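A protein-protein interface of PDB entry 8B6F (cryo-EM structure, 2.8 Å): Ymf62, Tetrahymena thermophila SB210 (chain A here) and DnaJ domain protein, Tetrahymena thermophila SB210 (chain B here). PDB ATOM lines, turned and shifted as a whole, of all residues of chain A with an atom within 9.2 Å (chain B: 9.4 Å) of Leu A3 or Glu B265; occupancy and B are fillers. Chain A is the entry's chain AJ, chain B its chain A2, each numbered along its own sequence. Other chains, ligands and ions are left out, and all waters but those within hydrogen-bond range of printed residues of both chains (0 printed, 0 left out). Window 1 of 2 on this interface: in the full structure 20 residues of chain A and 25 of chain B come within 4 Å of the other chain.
Leu A3 touches just these residues of chain B: Tyr B262 (3.95 Å) and Glu B265 (3.3 Å). Of the printed residues of chain B, Ile A13 touches Ile B294 (3.7 Å). Of the printed residues of chain B, Phe A16 touches Tyr B262 (3.9 Å). The nearest residue of chain A that does not touch Glu B265 is Ile A4 (5.8 Å).
Among the printed residues, pairs that only touch across the chains: Phe A2 with Glu B265, Phe A2 with Glu B268, Phe A2 with Gly B269, Leu A3 with Tyr B262, Ser A8 with Gly B292, Asn A12 with Ile B294, Ile A13 with Ile B294, Ile A14 with Ile B294, Phe A16 with Tyr B262, Asn A17 with Leu B266, Ile A20 with Tyr B262, Ile A24 with Tyr B262 and Ile A24 with Asn B263.
Of the 20 printed residues of chain B, 8 touch a printed residue of chain A. Among the printed residues, 15 pairs touch across the chains.
N of Leu A3 sits at hydrogen-bond distance from OE2 of Glu B265 (3.3 Å). OD1 of Asn A17 is in hydrogen-bond range of OH of Tyr B262, 3.1 Å away.
The side-chain hydroxyl (OG) of Ser A8 sits at hydrogen-bond distance from the backbone carbonyl oxygen (O) of Thr A5 (2.6 Å). The backbone carbonyl oxygen of Leu A3 lies within hydrogen-bond range of the side-chain hydroxyl of Thr A7 (2.9 Å). The backbone carbonyl oxygen (O) of Ser B259 lies within hydrogen-bond range of the side-chain amide nitrogen (ND2) of Asn B263.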
ATOM      1  N   PHE A   2      22.108   0.252 -14.607  1.00  0.00           N
ATOM      2  CA  PHE A   2      23.441  -0.044 -15.200  1.00  0.00           C
ATOM      3  C   PHE A   2      23.954  -1.401 -14.746  1.00  0.00           C
ATOM      4  O   PHE A   2      23.850  -1.757 -13.573  1.00  0.00           O
ATOM      5  CB  PHE A   2      24.449   1.044 -14.827  1.00  0.00           C
ATOM      6  CG  PHE A   2      24.748   1.997 -15.945  1.00  0.00           C
ATOM      7  CD1 PHE A   2      23.828   2.966 -16.310  1.00  0.00           C
ATOM      8  CD2 PHE A   2      25.951   1.931 -16.626  1.00  0.00           C
ATOM      9  CE1 PHE A   2      24.099   3.848 -17.339  1.00  0.00           C
ATOM     10  CE2 PHE A   2      26.231   2.808 -17.655  1.00  0.00           C
ATOM     11  CZ  PHE A   2      25.303   3.769 -18.013  1.00  0.00           C
ATOM     12  N   LEU A   3      24.511  -2.159 -15.691  1.00  0.00           N
ATOM     13  CA  LEU A   3      25.047  -3.475 -15.363  1.00  0.00           C
ATOM     14  C   LEU A   3      26.203  -3.363 -14.379  1.00  0.00           C
ATOM     15  O   LEU A   3      26.338  -4.192 -13.472  1.00  0.00           O
ATOM     16  CB  LEU A   3      25.489  -4.193 -16.638  1.00  0.00           C
ATOM     17  CG  LEU A   3      25.942  -5.646 -16.488  1.00  0.00           C
ATOM     18  CD1 LEU A   3      24.812  -6.522 -15.966  1.00  0.00           C
ATOM     19  CD2 LEU A   3      26.462  -6.175 -17.813  1.00  0.00           C
ATOM     20  N   ILE A   4      27.051  -2.346 -14.543  1.00  0.00           N
ATOM     21  CA  ILE A   4      28.163  -2.158 -13.617  1.00  0.00           C
ATOM     22  C   ILE A   4      27.641  -1.902 -12.209  1.00  0.00           C
ATOM     23  O   ILE A   4      28.142  -2.470 -11.232  1.00  0.00           O
ATOM     24  CB  ILE A   4      29.086  -1.020 -14.100  1.00  0.00           C
ATOM     25  CG1 ILE A   4      28.330   0.314 -14.133  1.00  0.00           C
ATOM     26  CG2 ILE A   4      29.656  -1.366 -15.469  1.00  0.00           C
ATOM     27  CD1 ILE A   4      29.111   1.476 -14.728  1.00  0.00           C
ATOM     28  N   THR A   5      26.630  -1.039 -12.080  1.00  0.00           N
ATOM     29  CA  THR A   5      26.071  -0.756 -10.762  1.00  0.00           C
ATOM     30  C   THR A   5      25.446  -2.003 -10.150  1.00  0.00           C
ATOM     31  O   THR A   5      25.630  -2.277  -8.959  1.00  0.00           O
ATOM     32  CB  THR A   5      25.035   0.365 -10.865  1.00  0.00           C
ATOM     33  OG1 THR A   5      25.660   1.555 -11.362  1.00  0.00           O
ATOM     34  CG2 THR A   5      24.410   0.657  -9.505  1.00  0.00           C
ATOM     35  N   ILE A   6      24.707  -2.774 -10.948  1.00  0.00           N
ATOM     36  CA  ILE A   6      24.075  -3.985 -10.431  1.00  0.00           C
ATOM     37  C   ILE A   6      25.130  -4.979  -9.965  1.00  0.00           C
ATOM     38  O   ILE A   6      24.995  -5.598  -8.903  1.00  0.00           O
ATOM     39  CB  ILE A   6      23.146  -4.597 -11.497  1.00  0.00           C
ATOM     40  CG1 ILE A   6      21.951  -3.671 -11.744  1.00  0.00           C
ATOM     41  CG2 ILE A   6      22.664  -5.981 -11.067  1.00  0.00           C
ATOM     42  CD1 ILE A   6      21.074  -4.083 -12.913  1.00  0.00           C
ATOM     43  N   THR A   7      26.197  -5.148 -10.748  1.00  0.00           N
ATOM     44  CA  THR A   7      27.222  -6.120 -10.387  1.00  0.00           C
ATOM     45  C   THR A   7      28.027  -5.674  -9.173  1.00  0.00           C
ATOM     46  O   THR A   7      28.493  -6.518  -8.401  1.00  0.00           O
ATOM     47  CB  THR A   7      28.153  -6.369 -11.574  1.00  0.00           C
ATOM     48  OG1 THR A   7      28.666  -5.119 -12.057  1.00  0.00           O
ATOM     49  CG2 THR A   7      27.412  -7.084 -12.695  1.00  0.00           C
ATOM     50  N   SER A   8      28.209  -4.365  -8.990  1.00  0.00           N
ATOM     51  CA  SER A   8      29.069  -3.882  -7.917  1.00  0.00           C
ATOM     52  C   SER A   8      28.579  -4.308  -6.538  1.00  0.00           C
ATOM     53  O   SER A   8      29.356  -4.265  -5.577  1.00  0.00           O
ATOM     54  CB  SER A   8      29.173  -2.356  -7.978  1.00  0.00           C
ATOM     55  OG  SER A   8      27.907  -1.748  -7.793  1.00  0.00           O
ATOM     56  N   TYR A   9      27.313  -4.716  -6.413  1.00  0.00           N
ATOM     57  CA  TYR A   9      26.774  -5.088  -5.109  1.00  0.00           C
ATOM     58  C   TYR A   9      27.323  -6.413  -4.598  1.00  0.00           C
ATOM     59  O   TYR A   9      27.317  -6.638  -3.384  1.00  0.00           O
ATOM     60  CB  TYR A   9      25.247  -5.160  -5.173  1.00  0.00           C
ATOM     61  CG  TYR A   9      24.571  -3.845  -5.494  1.00  0.00           C
ATOM     62  CD1 TYR A   9      25.114  -2.636  -5.070  1.00  0.00           C
ATOM     63  CD2 TYR A   9      23.388  -3.812  -6.220  1.00  0.00           C
ATOM     64  CE1 TYR A   9      24.496  -1.434  -5.360  1.00  0.00           C
ATOM     65  CE2 TYR A   9      22.762  -2.616  -6.515  1.00  0.00           C
ATOM     66  CZ  TYR A   9      23.321  -1.430  -6.083  1.00  0.00           C
ATOM     67  OH  TYR A   9      22.701  -0.237  -6.375  1.00  0.00           O
ATOM     68  N   PHE A  10      27.790  -7.295  -5.484  1.00  0.00           N
ATOM     69  CA  PHE A  10      28.316  -8.588  -5.069  1.00  0.00           C
ATOM     70  C   PHE A  10      29.638  -8.961  -5.722  1.00  0.00           C
ATOM     71  O   PHE A  10      30.289  -9.899  -5.249  1.00  0.00           O
ATOM     72  CB  PHE A  10      27.294  -9.702  -5.356  1.00  0.00           C
ATOM     73  CG  PHE A  10      26.988  -9.884  -6.814  1.00  0.00           C
ATOM     74  CD1 PHE A  10      26.017  -9.113  -7.433  1.00  0.00           C
ATOM     75  CD2 PHE A  10      27.660 -10.835  -7.565  1.00  0.00           C
ATOM     76  CE1 PHE A  10      25.729  -9.282  -8.774  1.00  0.00           C
ATOM     77  CE2 PHE A  10      27.377 -11.009  -8.907  1.00  0.00           C
ATOM     78  CZ  PHE A  10      26.409 -10.230  -9.513  1.00  0.00           C
ATOM     79  N   SER A  11      30.055  -8.275  -6.778  1.00  0.00           N
ATOM     80  CA  SER A  11      31.303  -8.582  -7.465  1.00  0.00           C
ATOM     81  C   SER A  11      31.655  -7.388  -8.344  1.00  0.00           C
ATOM     82  O   SER A  11      31.083  -6.303  -8.201  1.00  0.00           O
ATOM     83  CB  SER A  11      31.182  -9.884  -8.266  1.00  0.00           C
ATOM     84  OG  SER A  11      30.260  -9.748  -9.333  1.00  0.00           O
ATOM     85  N   ASN A  12      32.605  -7.584  -9.250  1.00  0.00           N
ATOM     86  CA  ASN A  12      32.998  -6.563 -10.209  1.00  0.00           C
ATOM     87  C   ASN A  12      32.506  -6.942 -11.599  1.00  0.00           C
ATOM     88  O   ASN A  12      32.398  -8.123 -11.940  1.00  0.00           O
ATOM     89  CB  ASN A  12      34.519  -6.370 -10.223  1.00  0.00           C
ATOM     90  CG  ASN A  12      35.276  -7.681 -10.281  1.00  0.00           C
ATOM     91  OD1 ASN A  12      34.833  -8.691  -9.737  1.00  0.00           O
ATOM     92  ND2 ASN A  12      36.427  -7.670 -10.944  1.00  0.00           N
ATOM     93  N   ILE A  13      32.198  -5.919 -12.399  1.00  0.00           N
ATOM     94  CA  ILE A  13      31.744  -6.154 -13.767  1.00  0.00           C
ATOM     95  C   ILE A  13      32.780  -6.951 -14.542  1.00  0.00           C
ATOM     96  O   ILE A  13      32.431  -7.754 -15.417  1.00  0.00           O
ATOM     97  CB  ILE A  13      31.425  -4.815 -14.463  1.00  0.00           C
ATOM     98  CG1 ILE A  13      30.902  -5.044 -15.885  1.00  0.00           C
ATOM     99  CG2 ILE A  13      32.658  -3.922 -14.506  1.00  0.00           C
ATOM    100  CD1 ILE A  13      29.621  -5.851 -15.956  1.00  0.00           C
ATOM    101  N   ILE A  14      34.062  -6.746 -14.245  1.00  0.00           N
ATOM    102  CA  ILE A  14      35.110  -7.490 -14.934  1.00  0.00           C
ATOM    103  C   ILE A  14      34.950  -8.982 -14.672  1.00  0.00           C
ATOM    104  O   ILE A  14      35.035  -9.806 -15.589  1.00  0.00           O
ATOM    105  CB  ILE A  14      36.497  -6.981 -14.501  1.00  0.00           C
ATOM    106  CG1 ILE A  14      36.629  -5.489 -14.825  1.00  0.00           C
ATOM    107  CG2 ILE A  14      37.597  -7.785 -15.188  1.00  0.00           C
ATOM    108  CD1 ILE A  14      37.936  -4.865 -14.387  1.00  0.00           C
ATOM    109  N   PHE A  16      32.158 -10.563 -13.606  1.00  0.00           N
ATOM    110  CA  PHE A  16      30.898 -11.040 -14.163  1.00  0.00           C
ATOM    111  C   PHE A  16      31.016 -11.266 -15.662  1.00  0.00           C
ATOM    112  O   PHE A  16      30.542 -12.279 -16.187  1.00  0.00           O
ATOM    113  CB  PHE A  16      29.774 -10.052 -13.856  1.00  0.00           C
ATOM    114  CG  PHE A  16      28.431 -10.497 -14.356  1.00  0.00           C
ATOM    115  CD1 PHE A  16      27.700 -11.449 -13.664  1.00  0.00           C
ATOM    116  CD2 PHE A  16      27.894  -9.956 -15.514  1.00  0.00           C
ATOM    117  CE1 PHE A  16      26.464 -11.860 -14.121  1.00  0.00           C
ATOM    118  CE2 PHE A  16      26.658 -10.363 -15.975  1.00  0.00           C
ATOM    119  CZ  PHE A  16      25.941 -11.316 -15.276  1.00  0.00           C
ATOM    120  N   ASN A  17      31.667 -10.338 -16.365  1.00  0.00           N
ATOM    121  CA  ASN A  17      31.898 -10.518 -17.793  1.00  0.00           C
ATOM    122  C   ASN A  17      32.809 -11.709 -18.059  1.00  0.00           C
ATOM    123  O   ASN A  17      32.536 -12.518 -18.953  1.00  0.00           O
ATOM    124  CB  ASN A  17      32.495  -9.245 -18.389  1.00  0.00           C
ATOM    125  CG  ASN A  17      32.712  -9.352 -19.882  1.00  0.00           C
ATOM    126  OD1 ASN A  17      31.841  -9.002 -20.674  1.00  0.00           O
ATOM    127  ND2 ASN A  17      33.883  -9.840 -20.275  1.00  0.00           N
ATOM    128  N   ILE A  20      30.506 -14.729 -17.885  1.00  0.00           N
ATOM    129  CA  ILE A  20      29.359 -14.873 -18.777  1.00  0.00           C
ATOM    130  C   ILE A  20      29.711 -14.684 -20.251  1.00  0.00           C
ATOM    131  O   ILE A  20      28.912 -15.067 -21.117  1.00  0.00           O
ATOM    132  CB  ILE A  20      28.236 -13.891 -18.375  1.00  0.00           C
ATOM    133  CG1 ILE A  20      26.930 -14.258 -19.086  1.00  0.00           C
ATOM    134  CG2 ILE A  20      28.627 -12.458 -18.710  1.00  0.00           C
ATOM    135  CD1 ILE A  20      25.727 -13.440 -18.647  1.00  0.00           C
ATOM    136  N   ILE A  24      27.969 -15.942 -23.855  1.00  0.00           N
ATOM    137  CA  ILE A  24      27.489 -14.917 -24.780  1.00  0.00           C
ATOM    138  C   ILE A  24      28.089 -15.135 -26.164  1.00  0.00           C
ATOM    139  O   ILE A  24      27.390 -15.071 -27.181  1.00  0.00           O
ATOM    140  CB  ILE A  24      27.808 -13.511 -24.238  1.00  0.00           C
ATOM    141  CG1 ILE A  24      26.985 -13.222 -22.978  1.00  0.00           C
ATOM    142  CG2 ILE A  24      27.559 -12.442 -25.305  1.00  0.00           C
ATOM    143  CD1 ILE A  24      25.489 -13.097 -23.204  1.00  0.00           C
ATOM    144  N   GLY B 257      18.956 -12.108 -29.679  1.00  0.00           N
ATOM    145  CA  GLY B 257      18.459 -11.102 -28.756  1.00  0.00           C
ATOM    146  C   GLY B 257      19.272 -11.031 -27.481  1.00  0.00           C
ATOM    147  O   GLY B 257      19.587  -9.944 -26.993  1.00  0.00           O
ATOM    148  N   VAL B 258      19.627 -12.191 -26.926  1.00  0.00           N
ATOM    149  CA  VAL B 258      20.427 -12.210 -25.705  1.00  0.00           C
ATOM    150  C   VAL B 258      21.804 -11.619 -25.966  1.00  0.00           C
ATOM    151  O   VAL B 258      22.296 -10.779 -25.204  1.00  0.00           O
ATOM    152  CB  VAL B 258      20.521 -13.639 -25.146  1.00  0.00           C
ATOM    153  CG1 VAL B 258      21.291 -13.633 -23.847  1.00  0.00           C
ATOM    154  CG2 VAL B 258      19.134 -14.226 -24.940  1.00  0.00           C
ATOM    155  N   SER B 259      22.448 -12.052 -27.051  1.00  0.00           N
ATOM    156  CA  SER B 259      23.775 -11.538 -27.368  1.00  0.00           C
ATOM    157  C   SER B 259      23.732 -10.034 -27.591  1.00  0.00           C
ATOM    158  O   SER B 259      24.606  -9.302 -27.112  1.00  0.00           O
ATOM    159  CB  SER B 259      24.337 -12.255 -28.597  1.00  0.00           C
ATOM    160  OG  SER B 259      23.482 -12.104 -29.716  1.00  0.00           O
ATOM    161  N   PHE B 260      22.727  -9.556 -28.324  1.00  0.00           N
ATOM    162  CA  PHE B 260      22.631  -8.126 -28.589  1.00  0.00           C
ATOM    163  C   PHE B 260      22.395  -7.336 -27.310  1.00  0.00           C
ATOM    164  O   PHE B 260      23.015  -6.288 -27.098  1.00  0.00           O
ATOM    165  CB  PHE B 260      21.509  -7.847 -29.585  1.00  0.00           C
ATOM    166  CG  PHE B 260      20.971  -6.450 -29.500  1.00  0.00           C
ATOM    167  CD1 PHE B 260      21.632  -5.399 -30.112  1.00  0.00           C
ATOM    168  CD2 PHE B 260      19.809  -6.187 -28.796  1.00  0.00           C
ATOM    169  CE1 PHE B 260      21.140  -4.113 -30.026  1.00  0.00           C
ATOM    170  CE2 PHE B 260      19.312  -4.905 -28.707  1.00  0.00           C
ATOM    171  CZ  PHE B 260      19.977  -3.867 -29.323  1.00  0.00           C
ATOM    172  N   LEU B 261      21.506  -7.820 -26.441  1.00  0.00           N
ATOM    173  CA  LEU B 261      21.228  -7.091 -25.209  1.00  0.00           C
ATOM    174  C   LEU B 261      22.471  -7.000 -24.338  1.00  0.00           C
ATOM    175  O   LEU B 261      22.796  -5.931 -23.810  1.00  0.00           O
ATOM    176  CB  LEU B 261      20.085  -7.765 -24.449  1.00  0.00           C
ATOM    177  CG  LEU B 261      18.689  -7.623 -25.063  1.00  0.00           C
ATOM    178  CD1 LEU B 261      17.684  -8.460 -24.291  1.00  0.00           C
ATOM    179  CD2 LEU B 261      18.247  -6.168 -25.108  1.00  0.00           C
ATOM    180  N   TYR B 262      23.186  -8.114 -24.175  1.00  0.00           N
ATOM    181  CA  TYR B 262      24.382  -8.084 -23.345  1.00  0.00           C
ATOM    182  C   TYR B 262      25.446  -7.180 -23.952  1.00  0.00           C
ATOM    183  O   TYR B 262      26.075  -6.385 -23.245  1.00  0.00           O
ATOM    184  CB  TYR B 262      24.917  -9.499 -23.143  1.00  0.00           C
ATOM    185  CG  TYR B 262      26.026  -9.561 -22.127  1.00  0.00           C
ATOM    186  CD1 TYR B 262      25.753  -9.504 -20.769  1.00  0.00           C
ATOM    187  CD2 TYR B 262      27.347  -9.666 -22.528  1.00  0.00           C
ATOM    188  CE1 TYR B 262      26.768  -9.554 -19.837  1.00  0.00           C
ATOM    189  CE2 TYR B 262      28.365  -9.718 -21.607  1.00  0.00           C
ATOM    190  CZ  TYR B 262      28.072  -9.661 -20.263  1.00  0.00           C
ATOM    191  OH  TYR B 262      29.093  -9.712 -19.346  1.00  0.00           O
ATOM    192  N   ASN B 263      25.662  -7.288 -25.265  1.00  0.00           N
ATOM    193  CA  ASN B 263      26.674  -6.464 -25.916  1.00  0.00           C
ATOM    194  C   ASN B 263      26.300  -4.989 -25.861  1.00  0.00           C
ATOM    195  O   ASN B 263      27.163  -4.130 -25.652  1.00  0.00           O
ATOM    196  CB  ASN B 263      26.868  -6.912 -27.363  1.00  0.00           C
ATOM    197  CG  ASN B 263      27.340  -8.347 -27.471  1.00  0.00           C
ATOM    198  OD1 ASN B 263      28.065  -8.841 -26.610  1.00  0.00           O
ATOM    199  ND2 ASN B 263      26.932  -9.024 -28.539  1.00  0.00           N
ATOM    200  N   MET B 264      25.015  -4.678 -26.041  1.00  0.00           N
ATOM    201  CA  MET B 264      24.570  -3.293 -25.952  1.00  0.00           C
ATOM    202  C   MET B 264      24.781  -2.740 -24.551  1.00  0.00           C
ATOM    203  O   MET B 264      25.208  -1.592 -24.385  1.00  0.00           O
ATOM    204  CB  MET B 264      23.100  -3.188 -26.354  1.00  0.00           C
ATOM    205  CG  MET B 264      22.535  -1.775 -26.293  1.00  0.00           C
ATOM    206  SD  MET B 264      20.801  -1.710 -26.780  1.00  0.00           S
ATOM    207  CE  MET B 264      20.478   0.048 -26.680  1.00  0.00           C
ATOM    208  N   GLU B 265      24.487  -3.541 -23.527  1.00  0.00           N
ATOM    209  CA  GLU B 265      24.719  -3.092 -22.160  1.00  0.00           C
ATOM    210  C   GLU B 265      26.201  -2.844 -21.910  1.00  0.00           C
ATOM    211  O   GLU B 265      26.573  -1.849 -21.276  1.00  0.00           O
ATOM    212  CB  GLU B 265      24.168  -4.126 -21.180  1.00  0.00           C
ATOM    213  CG  GLU B 265      24.016  -3.618 -19.761  1.00  0.00           C
ATOM    214  CD  GLU B 265      23.009  -2.493 -19.650  1.00  0.00           C
ATOM    215  OE1 GLU B 265      22.279  -2.245 -20.631  1.00  0.00           O
ATOM    216  OE2 GLU B 265      22.946  -1.855 -18.578  1.00  0.00           O
ATOM    217  N   LEU B 266      27.065  -3.739 -22.394  1.00  0.00           N
ATOM    218  CA  LEU B 266      28.500  -3.531 -22.233  1.00  0.00           C
ATOM    219  C   LEU B 266      28.951  -2.258 -22.934  1.00  0.00           C
ATOM    220  O   LEU B 266      29.724  -1.472 -22.374  1.00  0.00           O
ATOM    221  CB  LEU B 266      29.281  -4.728 -22.774  1.00  0.00           C
ATOM    222  CG  LEU B 266      29.230  -6.037 -21.991  1.00  0.00           C
ATOM    223  CD1 LEU B 266      30.052  -7.073 -22.733  1.00  0.00           C
ATOM    224  CD2 LEU B 266      29.728  -5.868 -20.567  1.00  0.00           C
ATOM    225  N   ASP B 267      28.472  -2.035 -24.158  1.00  0.00           N
ATOM    226  CA  ASP B 267      28.872  -0.844 -24.901  1.00  0.00           C
ATOM    227  C   ASP B 267      28.385   0.418 -24.206  1.00  0.00           C
ATOM    228  O   ASP B 267      29.111   1.416 -24.134  1.00  0.00           O
ATOM    229  CB  ASP B 267      28.332  -0.914 -26.328  1.00  0.00           C
ATOM    230  CG  ASP B 267      28.814  -2.143 -27.074  1.00  0.00           C
ATOM    231  OD1 ASP B 267      29.561  -2.946 -26.478  1.00  0.00           O
ATOM    232  OD2 ASP B 267      28.447  -2.306 -28.257  1.00  0.00           O
ATOM    233  N   GLU B 268      27.155   0.397 -23.692  1.00  0.00           N
ATOM    234  CA  GLU B 268      26.651   1.545 -22.950  1.00  0.00           C
ATOM    235  C   GLU B 268      27.501   1.810 -21.713  1.00  0.00           C
ATOM    236  O   GLU B 268      27.817   2.966 -21.404  1.00  0.00           O
ATOM    237  CB  GLU B 268      25.192   1.311 -22.560  1.00  0.00           C
ATOM    238  CG  GLU B 268      24.537   2.486 -21.858  1.00  0.00           C
ATOM    239  CD  GLU B 268      23.130   2.168 -21.393  1.00  0.00           C
ATOM    240  OE1 GLU B 268      22.669   1.033 -21.633  1.00  0.00           O
ATOM    241  OE2 GLU B 268      22.486   3.049 -20.786  1.00  0.00           O
ATOM    242  N   GLY B 269      27.877   0.754 -20.990  1.00  0.00           N
ATOM    243  CA  GLY B 269      28.726   0.937 -19.824  1.00  0.00           C
ATOM    244  C   GLY B 269      30.088   1.506 -20.173  1.00  0.00           C
ATOM    245  O   GLY B 269      30.592   2.399 -19.490  1.00  0.00           O
ATOM    246  N   LEU B 270      30.702   0.996 -21.242  1.00  0.00           N
ATOM    247  CA  LEU B 270      32.010   1.500 -21.650  1.00  0.00           C
ATOM    248  C   LEU B 270      31.925   2.960 -22.073  1.00  0.00           C
ATOM    249  O   LEU B 270      32.794   3.767 -21.725  1.00  0.00           O
ATOM    250  CB  LEU B 270      32.575   0.643 -22.781  1.00  0.00           C
ATOM    251  CG  LEU B 270      32.896  -0.807 -22.414  1.00  0.00           C
ATOM    252  CD1 LEU B 270      33.263  -1.599 -23.656  1.00  0.00           C
ATOM    253  CD2 LEU B 270      34.016  -0.876 -21.388  1.00  0.00           C
ATOM    254  N   GLY B 271      30.891   3.314 -22.835  1.00  0.00           N
ATOM    255  CA  GLY B 271      30.714   4.705 -23.215  1.00  0.00           C
ATOM    256  C   GLY B 271      30.475   5.603 -22.017  1.00  0.00           C
ATOM    257  O   GLY B 271      31.018   6.706 -21.937  1.00  0.00           O
ATOM    258  N   GLY B 272      29.671   5.136 -21.062  1.00  0.00           N
ATOM    259  CA  GLY B 272      29.453   5.912 -19.853  1.00  0.00           C
ATOM    260  C   GLY B 272      30.734   6.134 -19.072  1.00  0.00           C
ATOM    261  O   GLY B 272      30.997   7.238 -18.593  1.00  0.00           O
ATOM    262  N   LEU B 273      31.554   5.090 -18.943  1.00  0.00           N
ATOM    263  CA  LEU B 273      32.832   5.239 -18.256  1.00  0.00           C
ATOM    264  C   LEU B 273      33.735   6.217 -18.992  1.00  0.00           C
ATOM    265  O   LEU B 273      34.417   7.036 -18.366  1.00  0.00           O
ATOM    266  CB  LEU B 273      33.515   3.878 -18.114  1.00  0.00           C
ATOM    267  CG  LEU B 273      32.845   2.876 -17.170  1.00  0.00           C
ATOM    268  CD1 LEU B 273      33.524   1.522 -17.269  1.00  0.00           C
ATOM    269  CD2 LEU B 273      32.863   3.373 -15.734  1.00  0.00           C
ATOM    270  N   LYS B 276      32.417   9.697 -18.331  1.00  0.00           N
ATOM    271  CA  LYS B 276      32.635  10.070 -16.937  1.00  0.00           C
ATOM    272  C   LYS B 276      34.090  10.444 -16.684  1.00  0.00           C
ATOM    273  O   LYS B 276      34.373  11.424 -15.986  1.00  0.00           O
ATOM    274  CB  LYS B 276      32.204   8.930 -16.015  1.00  0.00           C
ATOM    275  CG  LYS B 276      30.696   8.774 -15.908  1.00  0.00           C
ATOM    276  CD  LYS B 276      30.311   7.568 -15.067  1.00  0.00           C
ATOM    277  CE  LYS B 276      28.799   7.383 -15.040  1.00  0.00           C
ATOM    278  NZ  LYS B 276      28.388   6.219 -14.206  1.00  0.00           N
ATOM    279  N   GLY B 292      32.033   1.662  -9.064  1.00  0.00           N
ATOM    280  CA  GLY B 292      31.581   0.280  -9.066  1.00  0.00           C
ATOM    281  C   GLY B 292      32.687  -0.724  -8.830  1.00  0.00           C
ATOM    282  O   GLY B 292      32.734  -1.761  -9.502  1.00  0.00           O
ATOM    283  N   ILE B 294      35.641  -0.530  -9.692  1.00  0.00           N
ATOM    284  CA  ILE B 294      36.487  -0.559 -10.877  1.00  0.00           C
ATOM    285  C   ILE B 294      37.316   0.714 -10.905  1.00  0.00           C
ATOM    286  O   ILE B 294      36.833   1.788 -10.526  1.00  0.00           O
ATOM    287  CB  ILE B 294      35.654  -0.692 -12.171  1.00  0.00           C
ATOM    288  CG1 ILE B 294      34.847  -1.995 -12.167  1.00  0.00           C
ATOM    289  CG2 ILE B 294      36.551  -0.624 -13.403  1.00  0.00           C
ATOM    290  CD1 ILE B 294      35.683  -3.254 -12.078  1.00  0.00           C
